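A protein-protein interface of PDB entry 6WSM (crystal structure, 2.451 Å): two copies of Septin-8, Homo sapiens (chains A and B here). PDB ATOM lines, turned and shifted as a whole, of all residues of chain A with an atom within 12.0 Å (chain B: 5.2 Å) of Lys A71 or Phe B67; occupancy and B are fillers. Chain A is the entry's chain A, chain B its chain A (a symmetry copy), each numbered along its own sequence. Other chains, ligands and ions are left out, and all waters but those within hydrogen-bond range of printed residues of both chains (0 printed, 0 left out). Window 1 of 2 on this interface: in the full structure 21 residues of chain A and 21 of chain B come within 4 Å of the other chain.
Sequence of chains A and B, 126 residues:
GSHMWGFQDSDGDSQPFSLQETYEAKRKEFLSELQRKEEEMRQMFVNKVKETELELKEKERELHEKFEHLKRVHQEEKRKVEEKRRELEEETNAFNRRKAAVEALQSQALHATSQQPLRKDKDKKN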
ATOM      1  N   GLU A  62      10.428  14.265   6.914  1.00  0.00           N
ATOM      2  CA  GLU A  62       9.371  14.540   7.882  1.00  0.00           C
ATOM      3  C   GLU A  62       9.899  14.455   9.308  1.00  0.00           C
ATOM      4  O   GLU A  62       9.488  15.236  10.175  1.00  0.00           O
ATOM      5  CB  GLU A  62       8.205  13.572   7.674  1.00  0.00           C
ATOM      6  CG  GLU A  62       6.983  13.861   8.538  1.00  0.00           C
ATOM      7  CD  GLU A  62       6.998  13.108   9.857  1.00  0.00           C
ATOM      8  OE1 GLU A  62       7.718  12.092   9.955  1.00  0.00           O
ATOM      9  OE2 GLU A  62       6.292  13.536  10.795  1.00  0.00           O
ATOM     10  N   LEU A  63      10.808  13.515   9.572  1.00  0.00           N
ATOM     11  CA  LEU A  63      11.431  13.443  10.888  1.00  0.00           C
ATOM     12  C   LEU A  63      12.430  14.570  11.105  1.00  0.00           C
ATOM     13  O   LEU A  63      12.745  14.887  12.257  1.00  0.00           O
ATOM     14  CB  LEU A  63      12.100  12.078  11.085  1.00  0.00           C
ATOM     15  CG  LEU A  63      13.069  11.533  10.032  1.00  0.00           C
ATOM     16  CD1 LEU A  63      14.490  12.035  10.255  1.00  0.00           C
ATOM     17  CD2 LEU A  63      13.036  10.009  10.016  1.00  0.00           C
ATOM     18  N   HIS A  64      12.929  15.185  10.029  1.00  0.00           N
ATOM     19  CA  HIS A  64      13.757  16.377  10.177  1.00  0.00           C
ATOM     20  C   HIS A  64      12.922  17.572  10.618  1.00  0.00           C
ATOM     21  O   HIS A  64      13.331  18.328  11.506  1.00  0.00           O
ATOM     22  CB  HIS A  64      14.481  16.686   8.867  1.00  0.00           C
ATOM     23  CG  HIS A  64      15.169  18.015   8.857  1.00  0.00           C
ATOM     24  ND1 HIS A  64      14.684  19.099   8.156  1.00  0.00           N
ATOM     25  CD2 HIS A  64      16.298  18.440   9.470  1.00  0.00           C
ATOM     26  CE1 HIS A  64      15.489  20.131   8.333  1.00  0.00           C
ATOM     27  NE2 HIS A  64      16.477  19.757   9.126  1.00  0.00           N
ATOM     28  N   GLU A  65      11.751  17.759  10.002  1.00  0.00           N
ATOM     29  CA  GLU A  65      10.864  18.843  10.412  1.00  0.00           C
ATOM     30  C   GLU A  65      10.367  18.635  11.836  1.00  0.00           C
ATOM     31  O   GLU A  65      10.284  19.588  12.620  1.00  0.00           O
ATOM     32  CB  GLU A  65       9.687  18.949   9.444  1.00  0.00           C
ATOM     33  CG  GLU A  65      10.097  19.171   8.000  1.00  0.00           C
ATOM     34  CD  GLU A  65      10.786  20.504   7.794  1.00  0.00           C
ATOM     35  OE1 GLU A  65      10.242  21.530   8.250  1.00  0.00           O
ATOM     36  OE2 GLU A  65      11.876  20.524   7.184  1.00  0.00           O
ATOM     37  N   LYS A  66      10.033  17.392  12.188  1.00  0.00           N
ATOM     38  CA  LYS A  66       9.584  17.090  13.542  1.00  0.00           C
ATOM     39  C   LYS A  66      10.703  17.222  14.564  1.00  0.00           C
ATOM     40  O   LYS A  66      10.422  17.407  15.753  1.00  0.00           O
ATOM     41  CB  LYS A  66       8.994  15.680  13.599  1.00  0.00           C
ATOM     42  N   PHE A  67      11.960  17.126  14.134  1.00  0.00           N
ATOM     43  CA  PHE A  67      13.085  17.305  15.041  1.00  0.00           C
ATOM     44  C   PHE A  67      13.473  18.772  15.189  1.00  0.00           C
ATOM     45  O   PHE A  67      13.803  19.215  16.295  1.00  0.00           O
ATOM     46  CB  PHE A  67      14.288  16.489  14.563  1.00  0.00           C
ATOM     47  CG  PHE A  67      15.513  16.677  15.403  1.00  0.00           C
ATOM     48  CD1 PHE A  67      15.507  16.328  16.743  1.00  0.00           C
ATOM     49  CD2 PHE A  67      16.672  17.198  14.855  1.00  0.00           C
ATOM     50  CE1 PHE A  67      16.632  16.500  17.523  1.00  0.00           C
ATOM     51  CE2 PHE A  67      17.802  17.371  15.629  1.00  0.00           C
ATOM     52  CZ  PHE A  67      17.782  17.022  16.965  1.00  0.00           C
ATOM     53  N   GLU A  68      13.440  19.536  14.094  1.00  0.00           N
ATOM     54  CA  GLU A  68      13.659  20.975  14.195  1.00  0.00           C
ATOM     55  C   GLU A  68      12.570  21.643  15.021  1.00  0.00           C
ATOM     56  O   GLU A  68      12.811  22.684  15.642  1.00  0.00           O
ATOM     57  CB  GLU A  68      13.724  21.601  12.801  1.00  0.00           C
ATOM     58  CG  GLU A  68      14.872  21.102  11.941  1.00  0.00           C
ATOM     59  CD  GLU A  68      16.230  21.410  12.540  1.00  0.00           C
ATOM     60  OE1 GLU A  68      16.398  22.509  13.108  1.00  0.00           O
ATOM     61  OE2 GLU A  68      17.128  20.548  12.448  1.00  0.00           O
ATOM     62  N   HIS A  69      11.367  21.063  15.036  1.00  0.00           N
ATOM     63  CA  HIS A  69      10.294  21.591  15.873  1.00  0.00           C
ATOM     64  C   HIS A  69      10.632  21.446  17.351  1.00  0.00           C
ATOM     65  O   HIS A  69      10.529  22.407  18.122  1.00  0.00           O
ATOM     66  CB  HIS A  69       8.981  20.879  15.546  1.00  0.00           C
ATOM     67  CG  HIS A  69       7.950  20.986  16.625  1.00  0.00           C
ATOM     68  ND1 HIS A  69       7.163  22.105  16.796  1.00  0.00           N
ATOM     69  CD2 HIS A  69       7.578  20.114  17.591  1.00  0.00           C
ATOM     70  CE1 HIS A  69       6.351  21.916  17.820  1.00  0.00           C
ATOM     71  NE2 HIS A  69       6.583  20.715  18.322  1.00  0.00           N
ATOM     72  N   LEU A  70      11.041  20.243  17.764  1.00  0.00           N
ATOM     73  CA  LEU A  70      11.357  20.013  19.170  1.00  0.00           C
ATOM     74  C   LEU A  70      12.594  20.786  19.609  1.00  0.00           C
ATOM     75  O   LEU A  70      12.723  21.119  20.792  1.00  0.00           O
ATOM     76  CB  LEU A  70      11.544  18.519  19.431  1.00  0.00           C
ATOM     77  CG  LEU A  70      10.282  17.666  19.297  1.00  0.00           C
ATOM     78  CD1 LEU A  70      10.567  16.219  19.670  1.00  0.00           C
ATOM     79  CD2 LEU A  70       9.163  18.235  20.153  1.00  0.00           C
ATOM     80  N   LYS A  71      13.515  21.072  18.684  1.00  0.00           N
ATOM     81  CA  LYS A  71      14.643  21.935  19.020  1.00  0.00           C
ATOM     82  C   LYS A  71      14.168  23.339  19.367  1.00  0.00           C
ATOM     83  O   LYS A  71      14.749  24.007  20.230  1.00  0.00           O
ATOM     84  CB  LYS A  71      15.644  21.981  17.865  1.00  0.00           C
ATOM     85  CG  LYS A  71      16.458  20.710  17.686  1.00  0.00           C
ATOM     86  CD  LYS A  71      17.503  20.849  16.577  1.00  0.00           C
ATOM     87  CE  LYS A  71      18.723  21.654  17.024  1.00  0.00           C
ATOM     88  NZ  LYS A  71      18.494  23.128  17.054  1.00  0.00           N
ATOM     89  N   ARG A  72      13.107  23.802  18.703  1.00  0.00           N
ATOM     90  CA  ARG A  72      12.552  25.118  19.001  1.00  0.00           C
ATOM     91  C   ARG A  72      11.761  25.109  20.302  1.00  0.00           C
ATOM     92  O   ARG A  72      11.833  26.064  21.082  1.00  0.00           O
ATOM     93  CB  ARG A  72      11.672  25.589  17.845  1.00  0.00           C
ATOM     94  N   VAL A  73      10.999  24.041  20.548  1.00  0.00           N
ATOM     95  CA  VAL A  73      10.269  23.919  21.805  1.00  0.00           C
ATOM     96  C   VAL A  73      11.240  23.792  22.972  1.00  0.00           C
ATOM     97  O   VAL A  73      11.006  24.342  24.055  1.00  0.00           O
ATOM     98  CB  VAL A  73       9.296  22.729  21.738  1.00  0.00           C
ATOM     99  CG1 VAL A  73       8.617  22.514  23.081  1.00  0.00           C
ATOM    100  CG2 VAL A  73       8.261  22.958  20.648  1.00  0.00           C
ATOM    101  N   HIS A  74      12.346  23.074  22.771  1.00  0.00           N
ATOM    102  CA  HIS A  74      13.366  22.973  23.810  1.00  0.00           C
ATOM    103  C   HIS A  74      14.000  24.330  24.087  1.00  0.00           C
ATOM    104  O   HIS A  74      14.127  24.748  25.245  1.00  0.00           O
ATOM    105  CB  HIS A  74      14.429  21.954  23.399  1.00  0.00           C
ATOM    106  CG  HIS A  74      15.671  22.012  24.230  1.00  0.00           C
ATOM    107  ND1 HIS A  74      15.699  21.632  25.554  1.00  0.00           N
ATOM    108  CD2 HIS A  74      16.928  22.413  23.926  1.00  0.00           C
ATOM    109  CE1 HIS A  74      16.921  21.793  26.030  1.00  0.00           C
ATOM    110  NE2 HIS A  74      17.686  22.267  25.062  1.00  0.00           N
ATOM    111  N   GLN A  75      14.407  25.037  23.029  1.00  0.00           N
ATOM    112  CA  GLN A  75      15.013  26.351  23.206  1.00  0.00           C
ATOM    113  C   GLN A  75      14.022  27.351  23.788  1.00  0.00           C
ATOM    114  O   GLN A  75      14.424  28.292  24.482  1.00  0.00           O
ATOM    115  CB  GLN A  75      15.560  26.860  21.872  1.00  0.00           C
ATOM    116  N   GLU A  76      12.728  27.165  23.521  1.00  0.00           N
ATOM    117  CA  GLU A  76      11.717  28.048  24.095  1.00  0.00           C
ATOM    118  C   GLU A  76      11.503  27.743  25.573  1.00  0.00           C
ATOM    119  O   GLU A  76      11.480  28.654  26.409  1.00  0.00           O
ATOM    120  CB  GLU A  76      10.406  27.917  23.320  1.00  0.00           C
ATOM    121  N   GLU A  77      11.341  26.460  25.914  1.00  0.00           N
ATOM    122  CA  GLU A  77      11.166  26.085  27.313  1.00  0.00           C
ATOM    123  C   GLU A  77      12.401  26.413  28.139  1.00  0.00           C
ATOM    124  O   GLU A  77      12.285  26.725  29.331  1.00  0.00           O
ATOM    125  CB  GLU A  77      10.834  24.596  27.424  1.00  0.00           C
ATOM    126  N   LYS A  78      13.589  26.352  27.533  1.00  0.00           N
ATOM    127  CA  LYS A  78      14.798  26.732  28.253  1.00  0.00           C
ATOM    128  C   LYS A  78      14.775  28.210  28.613  1.00  0.00           C
ATOM    129  O   LYS A  78      14.974  28.577  29.776  1.00  0.00           O
ATOM    130  CB  LYS A  78      16.040  26.404  27.428  1.00  0.00           C
ATOM    131  CG  LYS A  78      17.334  26.446  28.227  1.00  0.00           C
ATOM    132  CD  LYS A  78      18.480  25.806  27.463  1.00  0.00           C
ATOM    133  CE  LYS A  78      18.885  26.647  26.262  1.00  0.00           C
ATOM    134  NZ  LYS A  78      19.506  27.934  26.680  1.00  0.00           N
ATOM    135  N   ARG A  79      14.521  29.073  27.624  1.00  0.00           N
ATOM    136  CA  ARG A  79      14.464  30.507  27.885  1.00  0.00           C
ATOM    137  C   ARG A  79      13.368  30.850  28.883  1.00  0.00           C
ATOM    138  O   ARG A  79      13.474  31.852  29.599  1.00  0.00           O
ATOM    139  CB  ARG A  79      14.252  31.267  26.577  1.00  0.00           C
ATOM    140  N   LYS A  80      12.313  30.035  28.948  1.00  0.00           N
ATOM    141  CA  LYS A  80      11.251  30.272  29.921  1.00  0.00           C
ATOM    142  C   LYS A  80      11.754  30.048  31.342  1.00  0.00           C
ATOM    143  O   LYS A  80      11.506  30.864  32.238  1.00  0.00           O
ATOM    144  CB  LYS A  80      10.056  29.367  29.618  1.00  0.00           C
ATOM    145  CG  LYS A  80       8.857  29.592  30.520  1.00  0.00           C
ATOM    146  CD  LYS A  80       7.791  28.533  30.288  1.00  0.00           C
ATOM    147  CE  LYS A  80       6.627  28.698  31.253  1.00  0.00           C
ATOM    148  NZ  LYS A  80       5.698  27.532  31.192  1.00  0.00           N
ATOM    149  N   GLU A  82      14.969  29.991  32.173  1.00  0.00           N
ATOM    150  CA  GLU A  82      16.131  30.842  32.404  1.00  0.00           C
ATOM    151  C   GLU A  82      15.730  32.230  32.888  1.00  0.00           C
ATOM    152  O   GLU A  82      16.502  32.884  33.597  1.00  0.00           O
ATOM    153  CB  GLU A  82      16.971  30.941  31.131  1.00  0.00           C
ATOM    154  CG  GLU A  82      17.811  29.710  30.851  1.00  0.00           C
ATOM    155  CD  GLU A  82      18.632  29.843  29.584  1.00  0.00           C
ATOM    156  OE1 GLU A  82      18.301  30.710  28.746  1.00  0.00           O
ATOM    157  OE2 GLU A  82      19.613  29.083  29.432  1.00  0.00           O
ATOM    158  N   GLU B  62      17.495  18.970  33.627  1.00  0.00           N
ATOM    159  CA  GLU B  62      16.644  17.826  33.317  1.00  0.00           C
ATOM    160  C   GLU B  62      16.113  17.909  31.893  1.00  0.00           C
ATOM    161  O   GLU B  62      15.989  16.885  31.210  1.00  0.00           O
ATOM    162  CB  GLU B  62      15.495  17.741  34.324  1.00  0.00           C
ATOM    163  CG  GLU B  62      14.623  16.498  34.182  1.00  0.00           C
ATOM    164  CD  GLU B  62      13.428  16.714  33.269  1.00  0.00           C
ATOM    165  OE1 GLU B  62      13.045  17.884  33.056  1.00  0.00           O
ATOM    166  OE2 GLU B  62      12.876  15.713  32.766  1.00  0.00           O
ATOM    167  N   LEU B  63      15.792  19.118  31.426  1.00  0.00           N
ATOM    168  CA  LEU B  63      15.375  19.284  30.039  1.00  0.00           C
ATOM    169  C   LEU B  63      16.544  19.142  29.075  1.00  0.00           C
ATOM    170  O   LEU B  63      16.323  18.869  27.891  1.00  0.00           O
ATOM    171  CB  LEU B  63      14.675  20.634  29.852  1.00  0.00           C
ATOM    172  CG  LEU B  63      15.341  21.924  30.342  1.00  0.00           C
ATOM    173  CD1 LEU B  63      16.292  22.501  29.302  1.00  0.00           C
ATOM    174  CD2 LEU B  63      14.286  22.952  30.733  1.00  0.00           C
ATOM    175  N   HIS B  64      17.779  19.318  29.553  1.00  0.00           N
ATOM    176  CA  HIS B  64      18.941  19.032  28.718  1.00  0.00           C
ATOM    177  C   HIS B  64      19.108  17.532  28.508  1.00  0.00           C
ATOM    178  O   HIS B  64      19.372  17.083  27.388  1.00  0.00           O
ATOM    179  CB  HIS B  64      20.203  19.627  29.345  1.00  0.00           C
ATOM    180  CG  HIS B  64      21.469  19.187  28.681  1.00  0.00           C
ATOM    181  ND1 HIS B  64      22.332  18.274  29.252  1.00  0.00           N
ATOM    182  CD2 HIS B  64      22.016  19.526  27.490  1.00  0.00           C
ATOM    183  CE1 HIS B  64      23.357  18.076  28.443  1.00  0.00           C
ATOM    184  NE2 HIS B  64      23.190  18.824  27.367  1.00  0.00           N
ATOM    185  N   GLU B  65      18.961  16.745  29.578  1.00  0.00           N
ATOM    186  CA  GLU B  65      19.042  15.294  29.446  1.00  0.00           C
ATOM    187  C   GLU B  65      17.905  14.759  28.586  1.00  0.00           C
ATOM    188  O   GLU B  65      18.110  13.861  27.759  1.00  0.00           O
ATOM    189  CB  GLU B  65      19.019  14.642  30.828  1.00  0.00           C
ATOM    190  CG  GLU B  65      20.131  15.113  31.747  1.00  0.00           C
ATOM    191  CD  GLU B  65      21.504  14.719  31.242  1.00  0.00           C
ATOM    192  OE1 GLU B  65      21.694  13.531  30.908  1.00  0.00           O
ATOM    193  OE2 GLU B  65      22.389  15.598  31.171  1.00  0.00           O
ATOM    194  N   LYS B  66      16.699  15.301  28.764  1.00  0.00           N
ATOM    195  CA  LYS B  66      15.560  14.880  27.958  1.00  0.00           C
ATOM    196  C   LYS B  66      15.688  15.315  26.506  1.00  0.00           C
ATOM    197  O   LYS B  66      15.054  14.714  25.633  1.00  0.00           O
ATOM    198  CB  LYS B  66      14.262  15.430  28.552  1.00  0.00           C
ATOM    199  N   PHE B  67      16.485  16.346  26.228  1.00  0.00           N
ATOM    200  CA  PHE B  67      16.708  16.781  24.856  1.00  0.00           C
ATOM    201  C   PHE B  67      17.835  16.004  24.186  1.00  0.00           C
ATOM    202  O   PHE B  67      17.731  15.664  23.002  1.00  0.00           O
ATOM    203  CB  PHE B  67      17.008  18.280  24.816  1.00  0.00           C
ATOM    204  CG  PHE B  67      17.322  18.794  23.445  1.00  0.00           C
ATOM    205  CD1 PHE B  67      16.383  18.712  22.432  1.00  0.00           C
ATOM    206  CD2 PHE B  67      18.553  19.361  23.169  1.00  0.00           C
ATOM    207  CE1 PHE B  67      16.667  19.182  21.166  1.00  0.00           C
ATOM    208  CE2 PHE B  67      18.845  19.835  21.906  1.00  0.00           C
ATOM    209  CZ  PHE B  67      17.900  19.745  20.902  1.00  0.00           C
ATOM    210  N   GLU B  68      18.912  15.715  24.921  1.00  0.00           N
ATOM    211  CA  GLU B  68      19.959  14.852  24.384  1.00  0.00           C
ATOM    212  C   GLU B  68      19.434  13.449  24.114  1.00  0.00           C
ATOM    213  O   GLU B  68      19.948  12.752  23.233  1.00  0.00           O
ATOM    214  CB  GLU B  68      21.146  14.796  25.346  1.00  0.00           C
ATOM    215  CG  GLU B  68      21.835  16.131  25.573  1.00  0.00           C
ATOM    216  CD  GLU B  68      22.424  16.710  24.302  1.00  0.00           C
ATOM    217  OE1 GLU B  68      22.970  15.935  23.488  1.00  0.00           O
ATOM    218  OE2 GLU B  68      22.337  17.942  24.115  1.00  0.00           O
ATOM    219  N   HIS B  69      18.417  13.019  24.864  1.00  0.00           N
ATOM    220  CA  HIS B  69      17.799  11.722  24.610  1.00  0.00           C
ATOM    221  C   HIS B  69      17.102  11.703  23.256  1.00  0.00           C
ATOM    222  O   HIS B  69      17.310  10.790  22.449  1.00  0.00           O
ATOM    223  CB  HIS B  69      16.814  11.387  25.730  1.00  0.00           C
ATOM    224  CG  HIS B  69      15.802  10.350  25.355  1.00  0.00           C
ATOM    225  ND1 HIS B  69      16.081   9.000  25.359  1.00  0.00           N
ATOM    226  CD2 HIS B  69      14.512  10.465  24.962  1.00  0.00           C
ATOM    227  CE1 HIS B  69      15.007   8.330  24.986  1.00  0.00           C
ATOM    228  NE2 HIS B  69      14.039   9.196  24.738  1.00  0.00           N
ATOM    229  N   LEU B  70      16.270  12.713  22.988  1.00  0.00           N
ATOM    230  CA  LEU B  70      15.542  12.756  21.725  1.00  0.00           C
ATOM    231  C   LEU B  70      16.473  12.969  20.539  1.00  0.00           C
ATOM    232  O   LEU B  70      16.152  12.548  19.422  1.00  0.00           O
ATOM    233  CB  LEU B  70      14.475  13.849  21.767  1.00  0.00           C
ATOM    234  CG  LEU B  70      13.318  13.601  22.736  1.00  0.00           C
ATOM    235  CD1 LEU B  70      12.275  14.702  22.624  1.00  0.00           C
ATOM    236  CD2 LEU B  70      12.695  12.239  22.480  1.00  0.00           C
ATOM    237  N   LYS B  71      17.617  13.625  20.751  1.00  0.00           N
ATOM    238  CA  LYS B  71      18.610  13.725  19.685  1.00  0.00           C
ATOM    239  C   LYS B  71      19.151  12.352  19.315  1.00  0.00           C
ATOM    240  O   LYS B  71      19.457  12.087  18.147  1.00  0.00           O
ATOM    241  CB  LYS B  71      19.750  14.655  20.102  1.00  0.00           C
ATOM    242  CG  LYS B  71      19.384  16.131  20.126  1.00  0.00           C
ATOM    243  CD  LYS B  71      20.587  17.015  20.459  1.00  0.00           C
ATOM    244  CE  LYS B  71      21.529  17.193  19.268  1.00  0.00           C
ATOM    245  NZ  LYS B  71      22.408  16.015  19.014  1.00  0.00           N
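Among the printed residues, merely in contact across the chains: His A74 with Leu B63 (3.4 Å), His A74 with Phe B67 (3.5 Å), Phe A67 with Lys B71 (3.7 Å), Lys A71 with Phe B67 (3.7 Å) and Leu A70 with Leu B70 (3.7 Å).
Of chain B, only Phe B67 (3.7 Å) comes within 4 Å of Lys A71. Of chain A, only Lys A71 (3.7 Å) and His A74 (3.5 Å) come within 4 Å of Phe B67. No residue of chain A comes within 4 Å of His B64. No residue of chain A comes within 4 Å of Glu B65. No residue of chain A comes within 4 Å of Lys B66. No residue of chain A comes within 4 Å of Glu B68. Of the printed residues of chain B, Leu A70 touches Leu B70. Of the printed residues of chain A, Leu B63 touches His A74 (3.4 Å). Of the printed residues of chain B, Phe A67 touches Lys B71 (3.7 Å). Of the printed residues of chain B, His A74 touches Leu B63 and Phe B67. Glu A82 touches none of the printed residues of chain B. The nearest printed residue of chain B that does not touch Lys A71 is Lys B71 (5.7 Å). The nearest residue of chain A that does not touch Phe B67 is Leu A70 (4.4 Å). The nearest printed residue of chain B that does not touch His A74 is His B64 (4.4 Å).
Of the 20 printed residues of chain A, 4 touch a printed residue of chain B. Hydrophobic or aromatic side chains of chain A that line the printed part of chain B: Phe A67, Leu A70 and His A74. Of the 10 printed residues of chain B, 4 touch a printed residue of chain A. Among the printed residues, 5 pairs touch across the chains.
Phe A67 touches Lys B71, and with the chains exchanged Lys A71 touches Phe B67. Leu A70 touches its own counterpart, Leu B70. Of the 5 pairs that touch across the chains among the printed residues, 3 have their exchanged pair printed and touching as well.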
